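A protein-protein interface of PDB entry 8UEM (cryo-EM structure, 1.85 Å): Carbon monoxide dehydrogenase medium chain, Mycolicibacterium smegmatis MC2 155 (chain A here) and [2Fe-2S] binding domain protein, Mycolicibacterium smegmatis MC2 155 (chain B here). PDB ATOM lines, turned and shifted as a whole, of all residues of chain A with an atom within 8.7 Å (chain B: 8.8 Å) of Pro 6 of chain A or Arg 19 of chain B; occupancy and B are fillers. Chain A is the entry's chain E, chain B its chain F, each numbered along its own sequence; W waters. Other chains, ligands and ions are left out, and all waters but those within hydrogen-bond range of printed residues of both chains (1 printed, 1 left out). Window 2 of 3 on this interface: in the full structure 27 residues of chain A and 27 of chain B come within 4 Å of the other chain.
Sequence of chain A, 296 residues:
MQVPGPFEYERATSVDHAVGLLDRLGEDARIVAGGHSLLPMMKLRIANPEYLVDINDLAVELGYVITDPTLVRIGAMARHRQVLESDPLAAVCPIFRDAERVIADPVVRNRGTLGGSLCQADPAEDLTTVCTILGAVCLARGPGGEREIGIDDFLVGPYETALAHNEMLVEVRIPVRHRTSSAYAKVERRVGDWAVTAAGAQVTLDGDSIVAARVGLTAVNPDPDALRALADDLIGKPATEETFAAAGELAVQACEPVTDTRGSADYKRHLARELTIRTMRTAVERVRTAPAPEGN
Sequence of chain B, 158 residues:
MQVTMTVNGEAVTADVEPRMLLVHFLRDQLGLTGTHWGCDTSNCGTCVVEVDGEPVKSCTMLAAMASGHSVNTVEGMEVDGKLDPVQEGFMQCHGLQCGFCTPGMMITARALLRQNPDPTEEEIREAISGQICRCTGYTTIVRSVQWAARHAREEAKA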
ATOM      1  N   GLN A   2       9.118 -25.068  37.501  1.00  0.00           N
ATOM      2  CA  GLN A   2      10.554 -25.296  37.456  1.00  0.00           C
ATOM      3  C   GLN A   2      10.950 -25.717  36.049  1.00  0.00           C
ATOM      4  O   GLN A   2      10.317 -26.591  35.455  1.00  0.00           O
ATOM      5  CB  GLN A   2      10.959 -26.364  38.465  1.00  0.00           C
ATOM      6  CG  GLN A   2      10.849 -25.926  39.906  1.00  0.00           C
ATOM      7  CD  GLN A   2      11.142 -27.048  40.871  1.00  0.00           C
ATOM      8  OE1 GLN A   2      12.287 -27.463  41.025  1.00  0.00           O
ATOM      9  NE2 GLN A   2      10.106 -27.556  41.517  1.00  0.00           N
ATOM     10  N   VAL A   3      11.994 -25.095  35.519  1.00  0.00           N
ATOM     11  CA  VAL A   3      12.384 -25.319  34.130  1.00  0.00           C
ATOM     12  C   VAL A   3      13.853 -25.709  34.090  1.00  0.00           C
ATOM     13  O   VAL A   3      14.627 -25.400  35.009  1.00  0.00           O
ATOM     14  CB  VAL A   3      12.116 -24.073  33.254  1.00  0.00           C
ATOM     15  CG1 VAL A   3      10.622 -23.881  33.049  1.00  0.00           C
ATOM     16  CG2 VAL A   3      12.750 -22.847  33.877  1.00  0.00           C
ATOM     17  N   PRO A   4      14.267 -26.404  33.039  1.00  0.00           N
ATOM     18  CA  PRO A   4      15.655 -26.865  32.956  1.00  0.00           C
ATOM     19  C   PRO A   4      16.626 -25.709  32.778  1.00  0.00           C
ATOM     20  O   PRO A   4      16.283 -24.632  32.288  1.00  0.00           O
ATOM     21  CB  PRO A   4      15.656 -27.777  31.724  1.00  0.00           C
ATOM     22  CG  PRO A   4      14.213 -28.035  31.406  1.00  0.00           C
ATOM     23  CD  PRO A   4      13.461 -26.849  31.894  1.00  0.00           C
ATOM     24  N   GLY A   5      17.866 -25.954  33.185  1.00  0.00           N
ATOM     25  CA  GLY A   5      18.952 -25.075  32.835  1.00  0.00           C
ATOM     26  C   GLY A   5      19.258 -25.197  31.357  1.00  0.00           C
ATOM     27  O   GLY A   5      18.790 -26.117  30.681  1.00  0.00           O
ATOM     28  N   PRO A   6      20.041 -24.266  30.819  1.00  0.00           N
ATOM     29  CA  PRO A   6      20.370 -24.331  29.392  1.00  0.00           C
ATOM     30  C   PRO A   6      21.108 -25.616  29.050  1.00  0.00           C
ATOM     31  O   PRO A   6      21.880 -26.149  29.847  1.00  0.00           O
ATOM     32  CB  PRO A   6      21.257 -23.102  29.173  1.00  0.00           C
ATOM     33  CG  PRO A   6      20.941 -22.195  30.306  1.00  0.00           C
ATOM     34  CD  PRO A   6      20.615 -23.076  31.465  1.00  0.00           C
ATOM     35  N   PHE A   7      20.871 -26.105  27.838  1.00  0.00           N
ATOM     36  CA  PHE A   7      21.590 -27.295  27.322  1.00  0.00           C
ATOM     37  C   PHE A   7      21.519 -27.208  25.800  1.00  0.00           C
ATOM     38  O   PHE A   7      20.773 -26.387  25.278  1.00  0.00           O
ATOM     39  CB  PHE A   7      21.011 -28.611  27.858  1.00  0.00           C
ATOM     40  CG  PHE A   7      19.581 -28.901  27.483  1.00  0.00           C
ATOM     41  CD1 PHE A   7      19.271 -29.552  26.303  1.00  0.00           C
ATOM     42  CD2 PHE A   7      18.545 -28.530  28.322  1.00  0.00           C
ATOM     43  CE1 PHE A   7      17.957 -29.814  25.959  1.00  0.00           C
ATOM     44  CE2 PHE A   7      17.232 -28.806  27.983  1.00  0.00           C
ATOM     45  CZ  PHE A   7      16.941 -29.442  26.804  1.00  0.00           C
ATOM     46  N   GLU A   8      22.218 -28.097  25.121  1.00  0.00           N
ATOM     47  CA  GLU A   8      22.200 -28.095  23.647  1.00  0.00           C
ATOM     48  C   GLU A   8      21.391 -29.311  23.232  1.00  0.00           C
ATOM     49  O   GLU A   8      21.328 -30.283  23.978  1.00  0.00           O
ATOM     50  CB  GLU A   8      23.609 -28.009  23.044  1.00  0.00           C
ATOM     51  CG  GLU A   8      24.269 -26.671  23.301  1.00  0.00           C
ATOM     52  CD  GLU A   8      23.553 -25.513  22.630  1.00  0.00           C
ATOM     53  OE1 GLU A   8      23.005 -24.661  23.350  1.00  0.00           O
ATOM     54  OE2 GLU A   8      23.548 -25.471  21.384  1.00  0.00           O
ATOM     55  N   TYR A   9      20.711 -29.192  22.121  1.00  0.00           N
ATOM     56  CA  TYR A   9      19.824 -30.288  21.708  1.00  0.00           C
ATOM     57  C   TYR A   9      20.302 -30.883  20.394  1.00  0.00           C
ATOM     58  O   TYR A   9      20.628 -30.131  19.490  1.00  0.00           O
ATOM     59  CB  TYR A   9      18.399 -29.763  21.566  1.00  0.00           C
ATOM     60  CG  TYR A   9      17.382 -30.725  21.021  1.00  0.00           C
ATOM     61  CD1 TYR A   9      16.660 -31.546  21.866  1.00  0.00           C
ATOM     62  CD2 TYR A   9      17.109 -30.779  19.665  1.00  0.00           C
ATOM     63  CE1 TYR A   9      15.703 -32.413  21.377  1.00  0.00           C
ATOM     64  CE2 TYR A   9      16.162 -31.644  19.158  1.00  0.00           C
ATOM     65  CZ  TYR A   9      15.455 -32.458  20.018  1.00  0.00           C
ATOM     66  OH  TYR A   9      14.521 -33.298  19.512  1.00  0.00           O
ATOM     67  N   LEU A  39      13.648 -35.287  31.882  1.00  0.00           N
ATOM     68  CA  LEU A  39      13.128 -33.922  31.859  1.00  0.00           C
ATOM     69  C   LEU A  39      12.665 -33.452  33.227  1.00  0.00           C
ATOM     70  O   LEU A  39      12.966 -32.305  33.585  1.00  0.00           O
ATOM     71  CB  LEU A  39      12.013 -33.794  30.819  1.00  0.00           C
ATOM     72  CG  LEU A  39      12.471 -33.825  29.359  1.00  0.00           C
ATOM     73  CD1 LEU A  39      11.310 -33.566  28.427  1.00  0.00           C
ATOM     74  CD2 LEU A  39      13.594 -32.816  29.124  1.00  0.00           C
ATOM     75  N   MET A  42      15.854 -32.514  35.081  1.00  0.00           N
ATOM     76  CA  MET A  42      16.442 -31.262  34.615  1.00  0.00           C
ATOM     77  C   MET A  42      15.583 -30.069  35.009  1.00  0.00           C
ATOM     78  O   MET A  42      16.109 -29.011  35.363  1.00  0.00           O
ATOM     79  CB  MET A  42      16.658 -31.300  33.102  1.00  0.00           C
ATOM     80  CG  MET A  42      17.237 -32.601  32.588  1.00  0.00           C
ATOM     81  SD  MET A  42      17.361 -32.675  30.795  1.00  0.00           S
ATOM     82  CE  MET A  42      17.706 -30.971  30.381  1.00  0.00           C
ATOM     83  N   LYS A  43      14.262 -30.223  34.962  1.00  0.00           N
ATOM     84  CA  LYS A  43      13.384 -29.155  35.419  1.00  0.00           C
ATOM     85  C   LYS A  43      13.655 -28.834  36.879  1.00  0.00           C
ATOM     86  O   LYS A  43      13.637 -27.667  37.280  1.00  0.00           O
ATOM     87  CB  LYS A  43      11.920 -29.542  35.212  1.00  0.00           C
ATOM     88  CG  LYS A  43      11.440 -29.467  33.772  1.00  0.00           C
ATOM     89  CD  LYS A  43      10.258 -30.396  33.517  1.00  0.00           C
ATOM     90  CE  LYS A  43       8.967 -29.809  34.068  1.00  0.00           C
ATOM     91  NZ  LYS A  43       7.787 -30.666  33.785  1.00  0.00           N
ATOM     92  N   ARG A  45      16.511 -29.374  38.088  1.00  0.00           N
ATOM     93  CA  ARG A  45      17.929 -29.057  38.081  1.00  0.00           C
ATOM     94  C   ARG A  45      18.732 -30.069  38.880  1.00  0.00           C
ATOM     95  O   ARG A  45      19.848 -29.782  39.319  1.00  0.00           O
ATOM     96  CB  ARG A  45      18.167 -27.634  38.592  1.00  0.00           C
ATOM     97  CG  ARG A  45      18.084 -26.587  37.492  1.00  0.00           C
ATOM     98  CD  ARG A  45      17.386 -25.328  37.951  1.00  0.00           C
ATOM     99  NE  ARG A  45      16.760 -24.627  36.838  1.00  0.00           N
ATOM    100  CZ  ARG A  45      17.408 -23.861  35.974  1.00  0.00           C
ATOM    101  NH1 ARG A  45      18.712 -23.665  36.068  1.00  0.00           N
ATOM    102  NH2 ARG A  45      16.731 -23.274  34.992  1.00  0.00           N
ATOM    103  N   ALA A  47      19.392 -32.988  37.278  1.00  0.00           N
ATOM    104  CA  ALA A  47      20.188 -33.388  36.129  1.00  0.00           C
ATOM    105  C   ALA A  47      20.448 -32.160  35.274  1.00  0.00           C
ATOM    106  O   ALA A  47      19.524 -31.395  34.983  1.00  0.00           O
ATOM    107  CB  ALA A  47      19.474 -34.466  35.313  1.00  0.00           C
ATOM    108  N   ASN A  48      21.704 -31.956  34.898  1.00  0.00           N
ATOM    109  CA  ASN A  48      22.102 -30.808  34.083  1.00  0.00           C
ATOM    110  C   ASN A  48      23.011 -31.268  32.952  1.00  0.00           C
ATOM    111  O   ASN A  48      24.181 -30.887  32.880  1.00  0.00           O
ATOM    112  CB  ASN A  48      22.777 -29.749  34.949  1.00  0.00           C
ATOM    113  CG  ASN A  48      21.949 -29.383  36.165  1.00  0.00           C
ATOM    114  OD1 ASN A  48      21.190 -28.416  36.143  1.00  0.00           O
ATOM    115  ND2 ASN A  48      22.072 -30.169  37.226  1.00  0.00           N
ATOM    116  N   PRO A  49      22.500 -32.098  32.050  1.00  0.00           N
ATOM    117  CA  PRO A  49      23.294 -32.481  30.880  1.00  0.00           C
ATOM    118  C   PRO A  49      23.624 -31.264  30.031  1.00  0.00           C
ATOM    119  O   PRO A  49      22.806 -30.360  29.868  1.00  0.00           O
ATOM    120  CB  PRO A  49      22.377 -33.456  30.136  1.00  0.00           C
ATOM    121  CG  PRO A  49      20.997 -33.090  30.589  1.00  0.00           C
ATOM    122  CD  PRO A  49      21.140 -32.663  32.009  1.00  0.00           C
ATOM    123  N   GLU A  50      24.843 -31.239  29.492  1.00  0.00           N
ATOM    124  CA  GLU A  50      25.168 -30.204  28.518  1.00  0.00           C
ATOM    125  C   GLU A  50      24.445 -30.439  27.202  1.00  0.00           C
ATOM    126  O   GLU A  50      24.060 -29.482  26.525  1.00  0.00           O
ATOM    127  CB  GLU A  50      26.677 -30.132  28.291  1.00  0.00           C
ATOM    128  CG  GLU A  50      27.492 -30.155  29.569  1.00  0.00           C
ATOM    129  CD  GLU A  50      27.240 -28.945  30.443  1.00  0.00           C
ATOM    130  OE1 GLU A  50      26.079 -28.730  30.844  1.00  0.00           O
ATOM    131  OE2 GLU A  50      28.207 -28.206  30.738  1.00  0.00           O
ATOM    132  N   TYR A  51      24.200 -31.697  26.918  1.00  0.00           N
ATOM    133  CA  TYR A  51      23.592 -32.025  25.612  1.00  0.00           C
ATOM    134  C   TYR A  51      22.543 -33.111  25.780  1.00  0.00           C
ATOM    135  O   TYR A  51      22.731 -33.971  26.605  1.00  0.00           O
ATOM    136  CB  TYR A  51      24.636 -32.577  24.636  1.00  0.00           C
ATOM    137  CG  TYR A  51      25.937 -31.826  24.538  1.00  0.00           C
ATOM    138  CD1 TYR A  51      26.075 -30.750  23.678  1.00  0.00           C
ATOM    139  CD2 TYR A  51      27.034 -32.196  25.296  1.00  0.00           C
ATOM    140  CE1 TYR A  51      27.265 -30.053  23.583  1.00  0.00           C
ATOM    141  CE2 TYR A  51      28.234 -31.510  25.213  1.00  0.00           C
ATOM    142  CZ  TYR A  51      28.348 -30.434  24.353  1.00  0.00           C
ATOM    143  OH  TYR A  51      29.525 -29.749  24.259  1.00  0.00           O
ATOM    144  N   LEU A  52      21.448 -32.983  25.047  1.00  0.00           N
ATOM    145  CA  LEU A  52      20.465 -34.074  24.981  1.00  0.00           C
ATOM    146  C   LEU A  52      20.475 -34.614  23.568  1.00  0.00           C
ATOM    147  O   LEU A  52      20.298 -33.854  22.632  1.00  0.00           O
ATOM    148  CB  LEU A  52      19.032 -33.645  25.315  1.00  0.00           C
ATOM    149  CG  LEU A  52      18.743 -33.368  26.784  1.00  0.00           C
ATOM    150  CD1 LEU A  52      17.250 -33.187  26.992  1.00  0.00           C
ATOM    151  CD2 LEU A  52      19.269 -34.502  27.642  1.00  0.00           C
ATOM    152  N   MET B   1      17.470 -22.359  18.883  1.00  0.00           N
ATOM    153  CA  MET B   1      17.353 -23.368  17.803  1.00  0.00           C
ATOM    154  C   MET B   1      16.039 -23.202  17.067  1.00  0.00           C
ATOM    155  O   MET B   1      15.070 -22.735  17.664  1.00  0.00           O
ATOM    156  CB  MET B   1      17.470 -24.833  18.249  1.00  0.00           C
ATOM    157  CG  MET B   1      16.320 -25.354  19.068  1.00  0.00           C
ATOM    158  SD  MET B   1      16.515 -27.132  19.264  1.00  0.00           S
ATOM    159  CE  MET B   1      16.459 -27.653  17.551  1.00  0.00           C
ATOM    160  N   VAL B   3      12.723 -24.686  15.415  1.00  0.00           N
ATOM    161  CA  VAL B   3      11.808 -25.811  15.516  1.00  0.00           C
ATOM    162  C   VAL B   3      10.639 -25.547  14.589  1.00  0.00           C
ATOM    163  O   VAL B   3      10.163 -24.412  14.478  1.00  0.00           O
ATOM    164  CB  VAL B   3      11.310 -26.037  16.959  1.00  0.00           C
ATOM    165  CG1 VAL B   3      12.473 -26.303  17.892  1.00  0.00           C
ATOM    166  CG2 VAL B   3      10.496 -24.843  17.422  1.00  0.00           C
ATOM    167  N   VAL B  16      13.572 -21.241  19.351  1.00  0.00           N
ATOM    168  CA  VAL B  16      13.388 -21.564  20.758  1.00  0.00           C
ATOM    169  C   VAL B  16      14.707 -22.048  21.332  1.00  0.00           C
ATOM    170  O   VAL B  16      15.536 -22.635  20.632  1.00  0.00           O
ATOM    171  CB  VAL B  16      12.294 -22.633  20.980  1.00  0.00           C
ATOM    172  CG1 VAL B  16      11.030 -22.276  20.225  1.00  0.00           C
ATOM    173  CG2 VAL B  16      12.812 -23.998  20.583  1.00  0.00           C
ATOM    174  N   GLU B  17      14.901 -21.791  22.614  1.00  0.00           N
ATOM    175  CA  GLU B  17      15.986 -22.443  23.314  1.00  0.00           C
ATOM    176  C   GLU B  17      15.713 -23.942  23.381  1.00  0.00           C
ATOM    177  O   GLU B  17      14.560 -24.357  23.531  1.00  0.00           O
ATOM    178  CB  GLU B  17      16.157 -21.866  24.717  1.00  0.00           C
ATOM    179  CG  GLU B  17      16.254 -20.350  24.754  1.00  0.00           C
ATOM    180  CD  GLU B  17      16.518 -19.822  26.151  1.00  0.00           C
ATOM    181  OE1 GLU B  17      16.903 -20.624  27.025  1.00  0.00           O
ATOM    182  OE2 GLU B  17      16.342 -18.609  26.373  1.00  0.00           O
ATOM    183  N   PRO B  18      16.732 -24.813  23.198  1.00  0.00           N
ATOM    184  CA  PRO B  18      16.546 -26.251  23.348  1.00  0.00           C
ATOM    185  C   PRO B  18      15.796 -26.635  24.633  1.00  0.00           C
ATOM    186  O   PRO B  18      15.062 -27.561  24.603  1.00  0.00           O
ATOM    187  CB  PRO B  18      18.005 -26.732  23.430  1.00  0.00           C
ATOM    188  CG  PRO B  18      18.713 -25.871  22.437  1.00  0.00           C
ATOM    189  CD  PRO B  18      18.108 -24.519  22.709  1.00  0.00           C
ATOM    190  N   ARG B  19      15.987 -25.893  25.712  1.00  0.00           N
ATOM    191  CA  ARG B  19      15.385 -26.259  26.983  1.00  0.00           C
ATOM    192  C   ARG B  19      13.921 -25.860  27.089  1.00  0.00           C
ATOM    193  O   ARG B  19      13.271 -26.230  28.070  1.00  0.00           O
ATOM    194  CB  ARG B  19      16.159 -25.616  28.125  1.00  0.00           C
ATOM    195  CG  ARG B  19      15.900 -24.146  28.243  1.00  0.00           C
ATOM    196  CD  ARG B  19      16.657 -23.605  29.407  1.00  0.00           C
ATOM    197  NE  ARG B  19      16.822 -22.164  29.347  1.00  0.00           N
ATOM    198  CZ  ARG B  19      17.139 -21.427  30.397  1.00  0.00           C
ATOM    199  NH1 ARG B  19      17.304 -21.971  31.589  1.00  0.00           N
ATOM    200  NH2 ARG B  19      17.310 -20.119  30.247  1.00  0.00           N
ATOM    201  N   MET B  20      13.391 -25.124  26.120  1.00  0.00           N
ATOM    202  CA  MET B  20      12.018 -24.652  26.220  1.00  0.00           C
ATOM    203  C   MET B  20      11.057 -25.828  26.230  1.00  0.00           C
ATOM    204  O   MET B  20      10.965 -26.580  25.260  1.00  0.00           O
ATOM    205  CB  MET B  20      11.691 -23.704  25.072  1.00  0.00           C
ATOM    206  CG  MET B  20      10.627 -22.690  25.444  1.00  0.00           C
ATOM    207  SD  MET B  20       9.791 -21.934  24.041  1.00  0.00           S
ATOM    208  CE  MET B  20       8.894 -20.614  24.857  1.00  0.00           C
ATOM    209  N   LEU B  21      10.350 -25.990  27.343  1.00  0.00           N
ATOM    210  CA  LEU B  21       9.299 -26.989  27.412  1.00  0.00           C
ATOM    211  C   LEU B  21       8.192 -26.642  26.429  1.00  0.00           C
ATOM    212  O   LEU B  21       7.901 -25.472  26.170  1.00  0.00           O
ATOM    213  CB  LEU B  21       8.742 -27.079  28.832  1.00  0.00           C
ATOM    214  CG  LEU B  21       9.782 -27.297  29.930  1.00  0.00           C
ATOM    215  CD1 LEU B  21       9.158 -27.111  31.303  1.00  0.00           C
ATOM    216  CD2 LEU B  21      10.399 -28.669  29.793  1.00  0.00           C
ATOM    217  N   LEU B  22       7.563 -27.683  25.887  1.00  0.00           N
ATOM    218  CA  LEU B  22       6.521 -27.477  24.893  1.00  0.00           C
ATOM    219  C   LEU B  22       5.383 -26.640  25.453  1.00  0.00           C
ATOM    220  O   LEU B  22       4.797 -25.830  24.732  1.00  0.00           O
ATOM    221  CB  LEU B  22       5.993 -28.820  24.394  1.00  0.00           C
ATOM    222  CG  LEU B  22       4.859 -28.765  23.371  1.00  0.00           C
ATOM    223  CD1 LEU B  22       5.310 -28.137  22.054  1.00  0.00           C
ATOM    224  CD2 LEU B  22       4.286 -30.141  23.150  1.00  0.00           C
ATOM    225  N   VAL B  23       5.029 -26.839  26.725  1.00  0.00           N
ATOM    226  CA  VAL B  23       3.920 -26.074  27.289  1.00  0.00           C
ATOM    227  C   VAL B  23       4.228 -24.587  27.233  1.00  0.00           C
ATOM    228  O   VAL B  23       3.352 -23.768  26.936  1.00  0.00           O
ATOM    229  CB  VAL B  23       3.599 -26.526  28.726  1.00  0.00           C
ATOM    230  CG1 VAL B  23       4.815 -26.415  29.608  1.00  0.00           C
ATOM    231  CG2 VAL B  23       2.458 -25.678  29.284  1.00  0.00           C
ATOM    232  N   HIS B  24       5.470 -24.212  27.527  1.00  0.00           N
ATOM    233  CA  HIS B  24       5.841 -22.804  27.484  1.00  0.00           C
ATOM    234  C   HIS B  24       5.930 -22.293  26.051  1.00  0.00           C
ATOM    235  O   HIS B  24       5.595 -21.136  25.779  1.00  0.00           O
ATOM    236  CB  HIS B  24       7.156 -22.595  28.225  1.00  0.00           C
ATOM    237  CG  HIS B  24       7.040 -22.782  29.703  1.00  0.00           C
ATOM    238  ND1 HIS B  24       7.962 -23.492  30.440  1.00  0.00           N
ATOM    239  CD2 HIS B  24       6.100 -22.364  30.581  1.00  0.00           C
ATOM    240  CE1 HIS B  24       7.600 -23.495  31.709  1.00  0.00           C
ATOM    241  NE2 HIS B  24       6.473 -22.820  31.821  1.00  0.00           N
ATOM    242  N   PHE B  25       6.389 -23.131  25.123  1.00  0.00           N
ATOM    243  CA  PHE B  25       6.410 -22.723  23.724  1.00  0.00           C
ATOM    244  C   PHE B  25       5.000 -22.485  23.199  1.00  0.00           C
ATOM    245  O   PHE B  25       4.762 -21.540  22.442  1.00  0.00           O
ATOM    246  CB  PHE B  25       7.128 -23.766  22.879  1.00  0.00           C
ATOM    247  CG  PHE B  25       7.043 -23.506  21.411  1.00  0.00           C
ATOM    248  CD1 PHE B  25       7.751 -22.466  20.835  1.00  0.00           C
ATOM    249  CD2 PHE B  25       6.252 -24.298  20.603  1.00  0.00           C
ATOM    250  CE1 PHE B  25       7.673 -22.226  19.478  1.00  0.00           C
ATOM    251  CE2 PHE B  25       6.169 -24.063  19.248  1.00  0.00           C
ATOM    252  CZ  PHE B  25       6.880 -23.024  18.686  1.00  0.00           C
ATOM    253  N   SER B  58       2.717 -31.665  27.941  1.00  0.00           N
ATOM    254  CA  SER B  58       3.578 -30.721  27.241  1.00  0.00           C
ATOM    255  C   SER B  58       4.644 -30.141  28.153  1.00  0.00           C
ATOM    256  O   SER B  58       5.631 -29.594  27.659  1.00  0.00           O
ATOM    257  CB  SER B  58       2.749 -29.596  26.628  1.00  0.00           C
ATOM    258  OG  SER B  58       2.130 -28.818  27.632  1.00  0.00           O
ATOM    259  N   CYS B  59       4.452 -30.225  29.468  1.00  0.00           N
ATOM    260  CA  CYS B  59       5.490 -29.816  30.402  1.00  0.00           C
ATOM    261  C   CYS B  59       6.665 -30.779  30.409  1.00  0.00           C
ATOM    262  O   CYS B  59       7.739 -30.421  30.891  1.00  0.00           O
ATOM    263  CB  CYS B  59       4.917 -29.717  31.811  1.00  0.00           C
ATOM    264  SG  CYS B  59       4.790 -31.323  32.602  1.00  0.00           S
ATOM    265  N   MET B  61       7.843 -32.340  27.629  1.00  0.00           N
ATOM    266  CA  MET B  61       8.304 -32.427  26.256  1.00  0.00           C
ATOM    267  C   MET B  61       8.944 -31.099  25.904  1.00  0.00           C
ATOM    268  O   MET B  61       8.356 -30.045  26.149  1.00  0.00           O
ATOM    269  CB  MET B  61       7.154 -32.729  25.292  1.00  0.00           C
ATOM    270  CG  MET B  61       7.612 -33.163  23.918  1.00  0.00           C
ATOM    271  SD  MET B  61       6.396 -34.131  23.019  1.00  0.00           S
ATOM    272  CE  MET B  61       7.258 -34.345  21.464  1.00  0.00           C
ATOM    273  N   LEU B  62      10.137 -31.162  25.341  1.00  0.00           N
ATOM    274  CA  LEU B  62      10.778 -29.920  24.874  1.00  0.00           C
ATOM    275  C   LEU B  62      10.143 -29.525  23.547  1.00  0.00           C
ATOM    276  O   LEU B  62       9.724 -30.417  22.831  1.00  0.00           O
ATOM    277  CB  LEU B  62      12.272 -30.196  24.680  1.00  0.00           C
ATOM    278  CG  LEU B  62      13.050 -30.685  25.889  1.00  0.00           C
ATOM    279  CD1 LEU B  62      14.406 -31.204  25.442  1.00  0.00           C
ATOM    280  CD2 LEU B  62      13.206 -29.565  26.906  1.00  0.00           C
ATOM    281  N   ALA B  63       9.952 -28.240  23.314  1.00  0.00           N
ATOM    282  CA  ALA B  63       9.527 -27.771  22.003  1.00  0.00           C
ATOM    283  C   ALA B  63      10.411 -28.365  20.915  1.00  0.00           C
ATOM    284  O   ALA B  63       9.920 -28.810  19.873  1.00  0.00           O
ATOM    285  CB  ALA B  63       9.560 -26.244  21.954  1.00  0.00           C
ATOM    286  N   ALA B  64      11.705 -28.442  21.184  1.00  0.00           N
ATOM    287  CA  ALA B  64      12.679 -28.987  20.204  1.00  0.00           C
ATOM    288  C   ALA B  64      12.318 -30.427  19.856  1.00  0.00           C
ATOM    289  O   ALA B  64      12.555 -30.842  18.732  1.00  0.00           O
ATOM    290  CB  ALA B  64      14.042 -28.925  20.807  1.00  0.00           C
ATOM    291  N   MET B  65      11.791 -31.162  20.834  1.00  0.00           N
ATOM    292  CA  MET B  65      11.364 -32.561  20.638  1.00  0.00           C
ATOM    293  C   MET B  65      10.073 -32.594  19.831  1.00  0.00           C
ATOM    294  O   MET B  65       9.899 -33.528  19.093  1.00  0.00           O
ATOM    295  CB  MET B  65      11.137 -33.280  21.974  1.00  0.00           C
ATOM    296  CG  MET B  65      12.403 -33.565  22.756  1.00  0.00           C
ATOM    297  SD  MET B  65      12.070 -33.954  24.501  1.00  0.00           S
ATOM    298  CE  MET B  65      10.890 -35.284  24.312  1.00  0.00           C
HETATM  299  O   HOH W   1      18.718 -24.832  26.004  1.00  0.00           O
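NZ of Lys 43 of chain A lies within hydrogen-bond range of O of Cys 59 of chain B, at 2.9 Å.
The backbone carbonyl oxygen (O) of Ala 64 of chain B is in hydrogen-bond range of the side-chain hydroxyl (OH) of Tyr 9 of chain A (3.2 Å).
The backbone carbonyl oxygen of Pro 4 of chain A sits at hydrogen-bond distance from the guanidinium group of Arg 19 of chain B, 2.9 Å away.
O of Val 3 of chain A is in hydrogen-bond range of NE of Arg 45 of chain A (2.9 Å).
The backbone carbonyl oxygen of Pro 4 of chain A lies within hydrogen-bond range of the guanidinium group of Arg 45 of chain A.
The backbone NH (N) of Leu 62 of chain B is in hydrogen-bond range of the side-chain sulfur (SD) of Met 65 of chain B.
The backbone carbonyl oxygen of Glu 8 of chain A lies within hydrogen-bond range of the backbone NH of Leu 52 of chain A, 2.9 Å away.
CD1 of Leu 21 of chain B touches CG1 of Val 3 of chain A (3.95 Å).
Pro 6 of chain A touches Arg 19 of chain B (CD to NH1, 3.5 Å).
Phe 7 of chain A touches Arg 19 of chain B.
Tyr 9 of chain A touches Pro 18 of chain B.
Met 65 of chain B touches Tyr 9 of chain A.
Leu 62 of chain B touches Leu 39 of chain A.
Leu 21 of chain B touches Lys 43 of chain A (CD1 to CE, 3.9 Å).
Leu 62 of chain B touches Leu 52 of chain A.
Of chain B, only Arg 19 comes within 4 Å of Gly 5 of chain A.
Of the printed residues of chain B, Pro 6 of chain A touches Arg 19 (3.5 Å).
Printed residues of chain B within 4 Å of Tyr 9 of chain A: Met 1, Pro 18, Ala 64 and Met 65.
Glu 50 of chain A touches none of the printed residues of chain B.
Pro 18 of chain B touches just these residues of chain A: Phe 7 and Tyr 9.
Val 23 of chain B touches none of the printed residues of chain A.
Printed residues of chain A within 4 Å of Leu 62 of chain B: Phe 7 (3.4 Å), Leu 39 (3.9 Å) and Leu 52 (3.8 Å).
The nearest residue of chain B that does not touch Pro 6 of chain A is Glu 17 of chain B (5.4 Å).
Hydrophobic or aromatic side chains of chain B within 4 Å of the printed part of chain A: Met 1, Pro 18, Leu 21, His 24, Leu 62, Ala 64 and Met 65.
Along chain B the printed residues that touch a printed residue of chain A span positions 1 to 65.
Of the 18 printed residues of chain A, 10 touch a printed residue of chain B.
Printed residues of chain A that touch a printed residue of chain B: Val 3, Pro 4, Gly 5, Pro 6, Phe 7, Tyr 9, Leu 39, Lys 43, Arg 45 and Leu 52.
Among the printed residues, 18 pairs touch across the chains.
Among the printed residues, no Asp or Glu carboxylate lies within 4 Å of a Lys or Arg side-chain nitrogen of the other chain.
Water W1 lies within hydrogen-bond range of the backbone carbonyl oxygen (O) of Phe 7 of chain A (2.7 Å) and the backbone NH (N) of Arg 19 of chain B (2.9 Å).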
